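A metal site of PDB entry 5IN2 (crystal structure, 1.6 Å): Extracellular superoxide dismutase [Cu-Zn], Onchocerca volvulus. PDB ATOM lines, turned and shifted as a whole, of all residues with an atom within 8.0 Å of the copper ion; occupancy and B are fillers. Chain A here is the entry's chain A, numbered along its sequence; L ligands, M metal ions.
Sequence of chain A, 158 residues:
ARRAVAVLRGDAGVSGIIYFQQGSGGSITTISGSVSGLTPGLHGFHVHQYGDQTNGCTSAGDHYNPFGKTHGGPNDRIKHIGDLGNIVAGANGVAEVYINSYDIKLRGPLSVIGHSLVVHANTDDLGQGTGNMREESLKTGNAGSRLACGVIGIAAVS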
ATOM      1  N   GLY A  44      32.056  -2.716   3.107  1.00  0.00           N
ATOM      2  CA  GLY A  44      31.203  -1.552   3.166  1.00  0.00           C
ATOM      3  C   GLY A  44      31.960  -0.289   3.573  1.00  0.00           C
ATOM      4  O   GLY A  44      32.900  -0.369   4.352  1.00  0.00           O
ATOM      5  N   PHE A  45      31.537   0.847   3.036  1.00  0.00           N
ATOM      6  CA  PHE A  45      32.306   2.098   3.098  1.00  0.00           C
ATOM      7  C   PHE A  45      31.323   3.230   3.219  1.00  0.00           C
ATOM      8  O   PHE A  45      30.545   3.465   2.296  1.00  0.00           O
ATOM      9  CB  PHE A  45      33.142   2.176   1.832  1.00  0.00           C
ATOM     10  CG  PHE A  45      34.257   3.201   1.835  1.00  0.00           C
ATOM     11  CD1 PHE A  45      35.249   3.158   2.781  1.00  0.00           C
ATOM     12  CD2 PHE A  45      34.378   4.091   0.781  1.00  0.00           C
ATOM     13  CE1 PHE A  45      36.322   4.052   2.714  1.00  0.00           C
ATOM     14  CE2 PHE A  45      35.435   4.973   0.716  1.00  0.00           C
ATOM     15  CZ  PHE A  45      36.400   4.942   1.698  1.00  0.00           C
ATOM     16  N   HIS A  46      31.278   3.903   4.360  1.00  0.00           N
ATOM     17  CA  HIS A  46      30.262   4.908   4.608  1.00  0.00           C
ATOM     18  C   HIS A  46      30.789   6.116   5.336  1.00  0.00           C
ATOM     19  O   HIS A  46      31.658   5.992   6.168  1.00  0.00           O
ATOM     20  CB  HIS A  46      29.123   4.396   5.479  1.00  0.00           C
ATOM     21  CG  HIS A  46      28.659   3.001   5.184  1.00  0.00           C
ATOM     22  ND1 HIS A  46      28.632   2.035   6.164  1.00  0.00           N
ATOM     23  CD2 HIS A  46      28.149   2.436   4.056  1.00  0.00           C
ATOM     24  CE1 HIS A  46      28.167   0.909   5.641  1.00  0.00           C
ATOM     25  NE2 HIS A  46      27.860   1.123   4.379  1.00  0.00           N
ATOM     26  N   VAL A  47      30.219   7.268   5.024  1.00  0.00           N
ATOM     27  CA  VAL A  47      30.340   8.435   5.908  1.00  0.00           C
ATOM     28  C   VAL A  47      29.232   8.349   6.961  1.00  0.00           C
ATOM     29  O   VAL A  47      28.036   8.256   6.638  1.00  0.00           O
ATOM     30  CB  VAL A  47      30.242   9.756   5.140  1.00  0.00           C
ATOM     31  CG1 VAL A  47      30.380  10.952   6.102  1.00  0.00           C
ATOM     32  CG2 VAL A  47      31.281   9.847   4.074  1.00  0.00           C
ATOM     33  N   HIS A  48      29.629   8.372   8.232  1.00  0.00           N
ATOM     34  CA  HIS A  48      28.704   8.272   9.340  1.00  0.00           C
ATOM     35  C   HIS A  48      28.404   9.641   9.897  1.00  0.00           C
ATOM     36  O   HIS A  48      29.081  10.608   9.541  1.00  0.00           O
ATOM     37  CB  HIS A  48      29.274   7.320  10.413  1.00  0.00           C
ATOM     38  CG  HIS A  48      29.086   5.867  10.084  1.00  0.00           C
ATOM     39  ND1 HIS A  48      28.346   5.020  10.874  1.00  0.00           N
ATOM     40  CD2 HIS A  48      29.526   5.127   9.041  1.00  0.00           C
ATOM     41  CE1 HIS A  48      28.350   3.804  10.349  1.00  0.00           C
ATOM     42  NE2 HIS A  48      29.054   3.843   9.235  1.00  0.00           N
ATOM     43  N   CYS A  57      35.023   3.522  16.873  1.00  0.00           N
ATOM     44  CA  CYS A  57      34.154   3.807  15.717  1.00  0.00           C
ATOM     45  C   CYS A  57      32.669   3.687  16.058  1.00  0.00           C
ATOM     46  O   CYS A  57      31.812   4.115  15.293  1.00  0.00           O
ATOM     47  CB  CYS A  57      34.484   2.865  14.559  1.00  0.00           C
ATOM     48  SG  CYS A  57      36.177   2.908  13.997  1.00  0.00           S
ATOM     49  N   ALA A  60      30.597   6.967  16.114  1.00  0.00           N
ATOM     50  CA  ALA A  60      30.349   7.624  14.843  1.00  0.00           C
ATOM     51  C   ALA A  60      28.857   7.672  14.503  1.00  0.00           C
ATOM     52  O   ALA A  60      28.454   8.352  13.585  1.00  0.00           O
ATOM     53  CB  ALA A  60      31.091   6.940  13.753  1.00  0.00           C
ATOM     54  N   GLY A  61      28.042   6.928  15.237  1.00  0.00           N
ATOM     55  CA  GLY A  61      26.610   6.935  14.990  1.00  0.00           C
ATOM     56  C   GLY A  61      26.238   6.215  13.708  1.00  0.00           C
ATOM     57  O   GLY A  61      26.979   5.370  13.218  1.00  0.00           O
ATOM     58  N   ASP A  62      25.049   6.528  13.209  1.00  0.00           N
ATOM     59  CA  ASP A  62      24.532   5.886  12.004  1.00  0.00           C
ATOM     60  C   ASP A  62      25.049   6.547  10.734  1.00  0.00           C
ATOM     61  O   ASP A  62      25.966   7.337  10.766  1.00  0.00           O
ATOM     62  CB  ASP A  62      23.017   5.907  12.058  1.00  0.00           C
ATOM     63  CG  ASP A  62      22.469   5.172  13.268  1.00  0.00           C
ATOM     64  OD1 ASP A  62      23.059   4.126  13.636  1.00  0.00           O
ATOM     65  OD2 ASP A  62      21.492   5.662  13.857  1.00  0.00           O
ATOM     66  N   HIS A  63      24.517   6.174   9.574  1.00  0.00           N
ATOM     67  CA  HIS A  63      25.028   6.767   8.344  1.00  0.00           C
ATOM     68  C   HIS A  63      24.615   8.218   8.254  1.00  0.00           C
ATOM     69  O   HIS A  63      23.521   8.573   8.676  1.00  0.00           O
ATOM     70  CB  HIS A  63      24.506   6.028   7.125  1.00  0.00           C
ATOM     71  CG  HIS A  63      24.931   4.595   7.077  1.00  0.00           C
ATOM     72  ND1 HIS A  63      24.637   3.757   6.023  1.00  0.00           N
ATOM     73  CD2 HIS A  63      25.640   3.851   7.958  1.00  0.00           C
ATOM     74  CE1 HIS A  63      25.131   2.555   6.258  1.00  0.00           C
ATOM     75  NE2 HIS A  63      25.756   2.585   7.427  1.00  0.00           N
ATOM     76  N   TYR A  64      25.458   9.036   7.636  1.00  0.00           N
ATOM     77  CA  TYR A  64      25.125  10.428   7.396  1.00  0.00           C
ATOM     78  C   TYR A  64      23.956  10.494   6.403  1.00  0.00           C
ATOM     79  O   TYR A  64      24.085  10.048   5.262  1.00  0.00           O
ATOM     80  CB  TYR A  64      26.342  11.190   6.879  1.00  0.00           C
ATOM     81  CG  TYR A  64      26.106  12.658   6.654  1.00  0.00           C
ATOM     82  CD1 TYR A  64      25.407  13.395   7.572  1.00  0.00           C
ATOM     83  CD2 TYR A  64      26.581  13.269   5.510  1.00  0.00           C
ATOM     84  CE1 TYR A  64      25.167  14.753   7.362  1.00  0.00           C
ATOM     85  CE2 TYR A  64      26.349  14.633   5.298  1.00  0.00           C
ATOM     86  CZ  TYR A  64      25.649  15.346   6.249  1.00  0.00           C
ATOM     87  OH  TYR A  64      25.387  16.691   6.074  1.00  0.00           O
ATOM     88  N   HIS A  71      18.753   3.480   3.175  1.00  0.00           N
ATOM     89  CA  HIS A  71      20.065   3.080   2.728  1.00  0.00           C
ATOM     90  C   HIS A  71      20.042   2.582   1.290  1.00  0.00           C
ATOM     91  O   HIS A  71      19.105   1.885   0.895  1.00  0.00           O
ATOM     92  CB  HIS A  71      20.602   1.982   3.639  1.00  0.00           C
ATOM     93  CG  HIS A  71      21.979   1.552   3.292  1.00  0.00           C
ATOM     94  ND1 HIS A  71      23.096   2.312   3.554  1.00  0.00           N
ATOM     95  CD2 HIS A  71      22.427   0.416   2.699  1.00  0.00           C
ATOM     96  CE1 HIS A  71      24.168   1.689   3.092  1.00  0.00           C
ATOM     97  NE2 HIS A  71      23.781   0.526   2.563  1.00  0.00           N
ATOM     98  N   GLY A  82      25.890   9.609   2.889  1.00  0.00           N
ATOM     99  CA  GLY A  82      27.117   8.940   3.252  1.00  0.00           C
ATOM    100  C   GLY A  82      27.360   7.571   2.653  1.00  0.00           C
ATOM    101  O   GLY A  82      28.374   6.934   2.938  1.00  0.00           O
ATOM    102  N   ASP A  83      26.450   7.089   1.816  1.00  0.00           N
ATOM    103  CA  ASP A  83      26.544   5.734   1.288  1.00  0.00           C
ATOM    104  C   ASP A  83      27.549   5.667   0.144  1.00  0.00           C
ATOM    105  O   ASP A  83      27.298   6.187  -0.936  1.00  0.00           O
ATOM    106  CB  ASP A  83      25.174   5.243   0.794  1.00  0.00           C
ATOM    107  CG  ASP A  83      24.232   4.947   1.908  1.00  0.00           C
ATOM    108  OD1 ASP A  83      24.656   4.741   3.085  1.00  0.00           O
ATOM    109  OD2 ASP A  83      23.011   4.888   1.655  1.00  0.00           O
ATOM    110  N   SER A 116      32.662  11.100  10.294  1.00  0.00           N
ATOM    111  CA  SER A 116      33.623  10.001  10.266  1.00  0.00           C
ATOM    112  C   SER A 116      33.430   9.166   9.017  1.00  0.00           C
ATOM    113  O   SER A 116      32.291   8.922   8.592  1.00  0.00           O
ATOM    114  CB  SER A 116      33.463   9.083  11.481  1.00  0.00           C
ATOM    115  OG  SER A 116      33.831   9.738  12.680  1.00  0.00           O
ATOM    116  N   LEU A 117      34.539   8.763   8.409  1.00  0.00           N
ATOM    117  CA  LEU A 117      34.556   7.742   7.349  1.00  0.00           C
ATOM    118  C   LEU A 117      34.832   6.408   8.006  1.00  0.00           C
ATOM    119  O   LEU A 117      35.737   6.304   8.846  1.00  0.00           O
ATOM    120  CB  LEU A 117      35.625   8.070   6.306  1.00  0.00           C
ATOM    121  CG  LEU A 117      35.760   7.144   5.112  1.00  0.00           C
ATOM    122  CD1 LEU A 117      34.484   7.226   4.282  1.00  0.00           C
ATOM    123  CD2 LEU A 117      36.965   7.558   4.271  1.00  0.00           C
ATOM    124  N   VAL A 118      34.090   5.365   7.615  1.00  0.00           N
ATOM    125  CA  VAL A 118      34.128   4.088   8.300  1.00  0.00           C
ATOM    126  C   VAL A 118      34.193   2.961   7.283  1.00  0.00           C
ATOM    127  O   VAL A 118      33.429   2.957   6.291  1.00  0.00           O
ATOM    128  CB  VAL A 118      32.882   3.875   9.179  1.00  0.00           C
ATOM    129  CG1 VAL A 118      32.967   2.513   9.919  1.00  0.00           C
ATOM    130  CG2 VAL A 118      32.689   5.021  10.192  1.00  0.00           C
ATOM    131  N   VAL A 119      35.108   2.018   7.499  1.00  0.00           N
ATOM    132  CA  VAL A 119      35.229   0.812   6.690  1.00  0.00           C
ATOM    133  C   VAL A 119      34.749  -0.384   7.483  1.00  0.00           C
ATOM    134  O   VAL A 119      35.053  -0.528   8.671  1.00  0.00           O
ATOM    135  CB  VAL A 119      36.684   0.557   6.233  1.00  0.00           C
ATOM    136  CG1 VAL A 119      36.737  -0.656   5.285  1.00  0.00           C
ATOM    137  CG2 VAL A 119      37.255   1.787   5.592  1.00  0.00           C
ATOM    138  N   HIS A 120      33.978  -1.260   6.850  1.00  0.00           N
ATOM    139  CA  HIS A 120      33.303  -2.337   7.541  1.00  0.00           C
ATOM    140  C   HIS A 120      33.876  -3.711   7.224  1.00  0.00           C
ATOM    141  O   HIS A 120      34.595  -3.876   6.256  1.00  0.00           O
ATOM    142  CB  HIS A 120      31.820  -2.325   7.174  1.00  0.00           C
ATOM    143  CG  HIS A 120      31.043  -1.227   7.813  1.00  0.00           C
ATOM    144  ND1 HIS A 120      30.370  -1.409   9.005  1.00  0.00           N
ATOM    145  CD2 HIS A 120      30.850   0.069   7.471  1.00  0.00           C
ATOM    146  CE1 HIS A 120      29.772  -0.283   9.349  1.00  0.00           C
ATOM    147  NE2 HIS A 120      30.050   0.630   8.430  1.00  0.00           N
ATOM    148  N   ASP A 124      28.475  -4.490   1.945  1.00  0.00           N
ATOM    149  CA  ASP A 124      27.268  -3.671   1.971  1.00  0.00           C
ATOM    150  C   ASP A 124      26.346  -4.183   0.870  1.00  0.00           C
ATOM    151  O   ASP A 124      26.734  -4.155  -0.297  1.00  0.00           O
ATOM    152  CB  ASP A 124      27.666  -2.211   1.744  1.00  0.00           C
ATOM    153  CG  ASP A 124      26.533  -1.221   1.838  1.00  0.00           C
ATOM    154  OD1 ASP A 124      25.345  -1.577   1.665  1.00  0.00           O
ATOM    155  OD2 ASP A 124      26.855  -0.024   2.067  1.00  0.00           O
ATOM    156  N   LYS A 139      18.721   0.106   6.539  1.00  0.00           N
ATOM    157  CA  LYS A 139      19.345   0.978   7.538  1.00  0.00           C
ATOM    158  C   LYS A 139      20.857   1.093   7.325  1.00  0.00           C
ATOM    159  O   LYS A 139      21.412   2.196   7.266  1.00  0.00           O
ATOM    160  CB  LYS A 139      19.067   0.450   8.940  1.00  0.00           C
ATOM    161  CG  LYS A 139      17.623   0.536   9.383  1.00  0.00           C
ATOM    162  CD  LYS A 139      17.434  -0.136  10.751  1.00  0.00           C
ATOM    163  CE  LYS A 139      15.973  -0.221  11.167  1.00  0.00           C
ATOM    164  NZ  LYS A 139      15.827  -0.914  12.484  1.00  0.00           N
ATOM    165  N   THR A 140      21.525  -0.049   7.229  1.00  0.00           N
ATOM    166  CA  THR A 140      22.995  -0.084   7.218  1.00  0.00           C
ATOM    167  C   THR A 140      23.639  -0.852   6.074  1.00  0.00           C
ATOM    168  O   THR A 140      24.840  -0.842   5.939  1.00  0.00           O
ATOM    169  CB  THR A 140      23.552  -0.732   8.498  1.00  0.00           C
ATOM    170  OG1 THR A 140      23.171  -2.115   8.507  1.00  0.00           O
ATOM    171  CG2 THR A 140      23.023  -0.030   9.732  1.00  0.00           C
ATOM    172  N   GLY A 141      22.849  -1.583   5.298  1.00  0.00           N
ATOM    173  CA  GLY A 141      23.419  -2.442   4.281  1.00  0.00           C
ATOM    174  C   GLY A 141      24.010  -3.758   4.800  1.00  0.00           C
ATOM    175  O   GLY A 141      24.645  -4.499   4.073  1.00  0.00           O
ATOM    176  N   ALA A 143      26.568  -4.445   6.634  1.00  0.00           N
ATOM    177  CA  ALA A 143      27.993  -4.567   6.357  1.00  0.00           C
ATOM    178  C   ALA A 143      28.813  -4.937   7.587  1.00  0.00           C
ATOM    179  O   ALA A 143      30.033  -5.006   7.510  1.00  0.00           O
ATOM    180  CB  ALA A 143      28.525  -3.291   5.757  1.00  0.00           C
ATOM    181  N   GLY A 144      28.167  -5.206   8.711  1.00  0.00           N
ATOM    182  CA  GLY A 144      28.867  -5.761   9.839  1.00  0.00           C
ATOM    183  C   GLY A 144      29.733  -4.755  10.561  1.00  0.00           C
ATOM    184  O   GLY A 144      29.500  -3.553  10.519  1.00  0.00           O
ATOM    185  N   SER A 145      30.725  -5.264  11.260  1.00  0.00           N
ATOM    186  CA  SER A 145      31.404  -4.451  12.249  1.00  0.00           C
ATOM    187  C   SER A 145      32.238  -3.355  11.607  1.00  0.00           C
ATOM    188  O   SER A 145      32.613  -3.431  10.428  1.00  0.00           O
ATOM    189  CB  SER A 145      32.264  -5.329  13.145  1.00  0.00           C
ATOM    190  OG  SER A 145      33.334  -5.875  12.418  1.00  0.00           O
ATOM    191  N   ARG A 146      32.533  -2.339  12.417  1.00  0.00           N
ATOM    192  CA  ARG A 146      33.323  -1.197  12.001  1.00  0.00           C
ATOM    193  C   ARG A 146      34.781  -1.499  12.293  1.00  0.00           C
ATOM    194  O   ARG A 146      35.189  -1.550  13.465  1.00  0.00           O
ATOM    195  CB  ARG A 146      32.886   0.060  12.742  1.00  0.00           C
ATOM    196  CG  ARG A 146      31.389   0.313  12.598  1.00  0.00           C
ATOM    197  CD  ARG A 146      30.883   1.484  13.366  1.00  0.00           C
ATOM    198  NE  ARG A 146      29.439   1.544  13.204  1.00  0.00           N
ATOM    199  CZ  ARG A 146      28.664   2.474  13.719  1.00  0.00           C
ATOM    200  NH1 ARG A 146      27.354   2.412  13.520  1.00  0.00           N
ATOM    201  NH2 ARG A 146      29.188   3.447  14.439  1.00  0.00           N
HETATM  202  S1  LIG L   1      26.720   0.620  10.389  1.00  0.00           S
HETATM  203  O1  LIG L   1      27.159   1.113   9.114  1.00  0.00           O
HETATM  204  O2  LIG L   1      27.764   0.610  11.417  1.00  0.00           O
HETATM  205  O3  LIG L   1      25.613   1.461  10.860  1.00  0.00           O
HETATM  206  O4  LIG L   1      26.281  -0.786  10.190  1.00  0.00           O
HETATM  207 CU    CU M   1      28.777   2.069   8.263  1.00  0.00          CU
HETATM  208 ZN    ZN M   2      23.482   4.117   4.418  1.00  0.00          ZN
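The backbone carbonyl oxygen of Gly 144 is in hydrogen-bond range of a ring nitrogen (ND1) of His 120.
The backbone NH of His 120 is in hydrogen-bond range of the backbone carbonyl oxygen of Gly 44, 2.9 Å away.
O of Ser 145 sits close to ND1 of His 120 (3.3 Å).
O of Asp 62 lies close to ND1 of His 48.
The backbone carbonyl oxygen (O) of Ser 116 lies within hydrogen-bond range of the backbone NH (N) of His 48.
ND1 of His 46 lies close to NE2 of His 63 (3.2 Å).
The backbone carbonyl oxygen of His 46 is in hydrogen-bond range of the backbone NH of Val 118, at 2.9 Å.
NE2 of His 46 lies within hydrogen-bond range of OD2 of Asp 124 (2.8 Å).
Residues that only touch the copper ion: His 63 (3.2 Å).
Of the 27 residues printed, 4 come within 4 Å of the copper ion.
The nearest printed residue that does not touch the copper ion is Val 118 (4.5 Å).
A ring nitrogen (NE2) of His 120 binds the copper ion (1.9 Å).
NE2 of His 48 is bound to the copper ion (2.0 Å).
The copper ion is bound by O1 of the ligand (2.1 Å).
A ring nitrogen (ND1) of His 46 binds the copper ion, at 2.1 Å.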
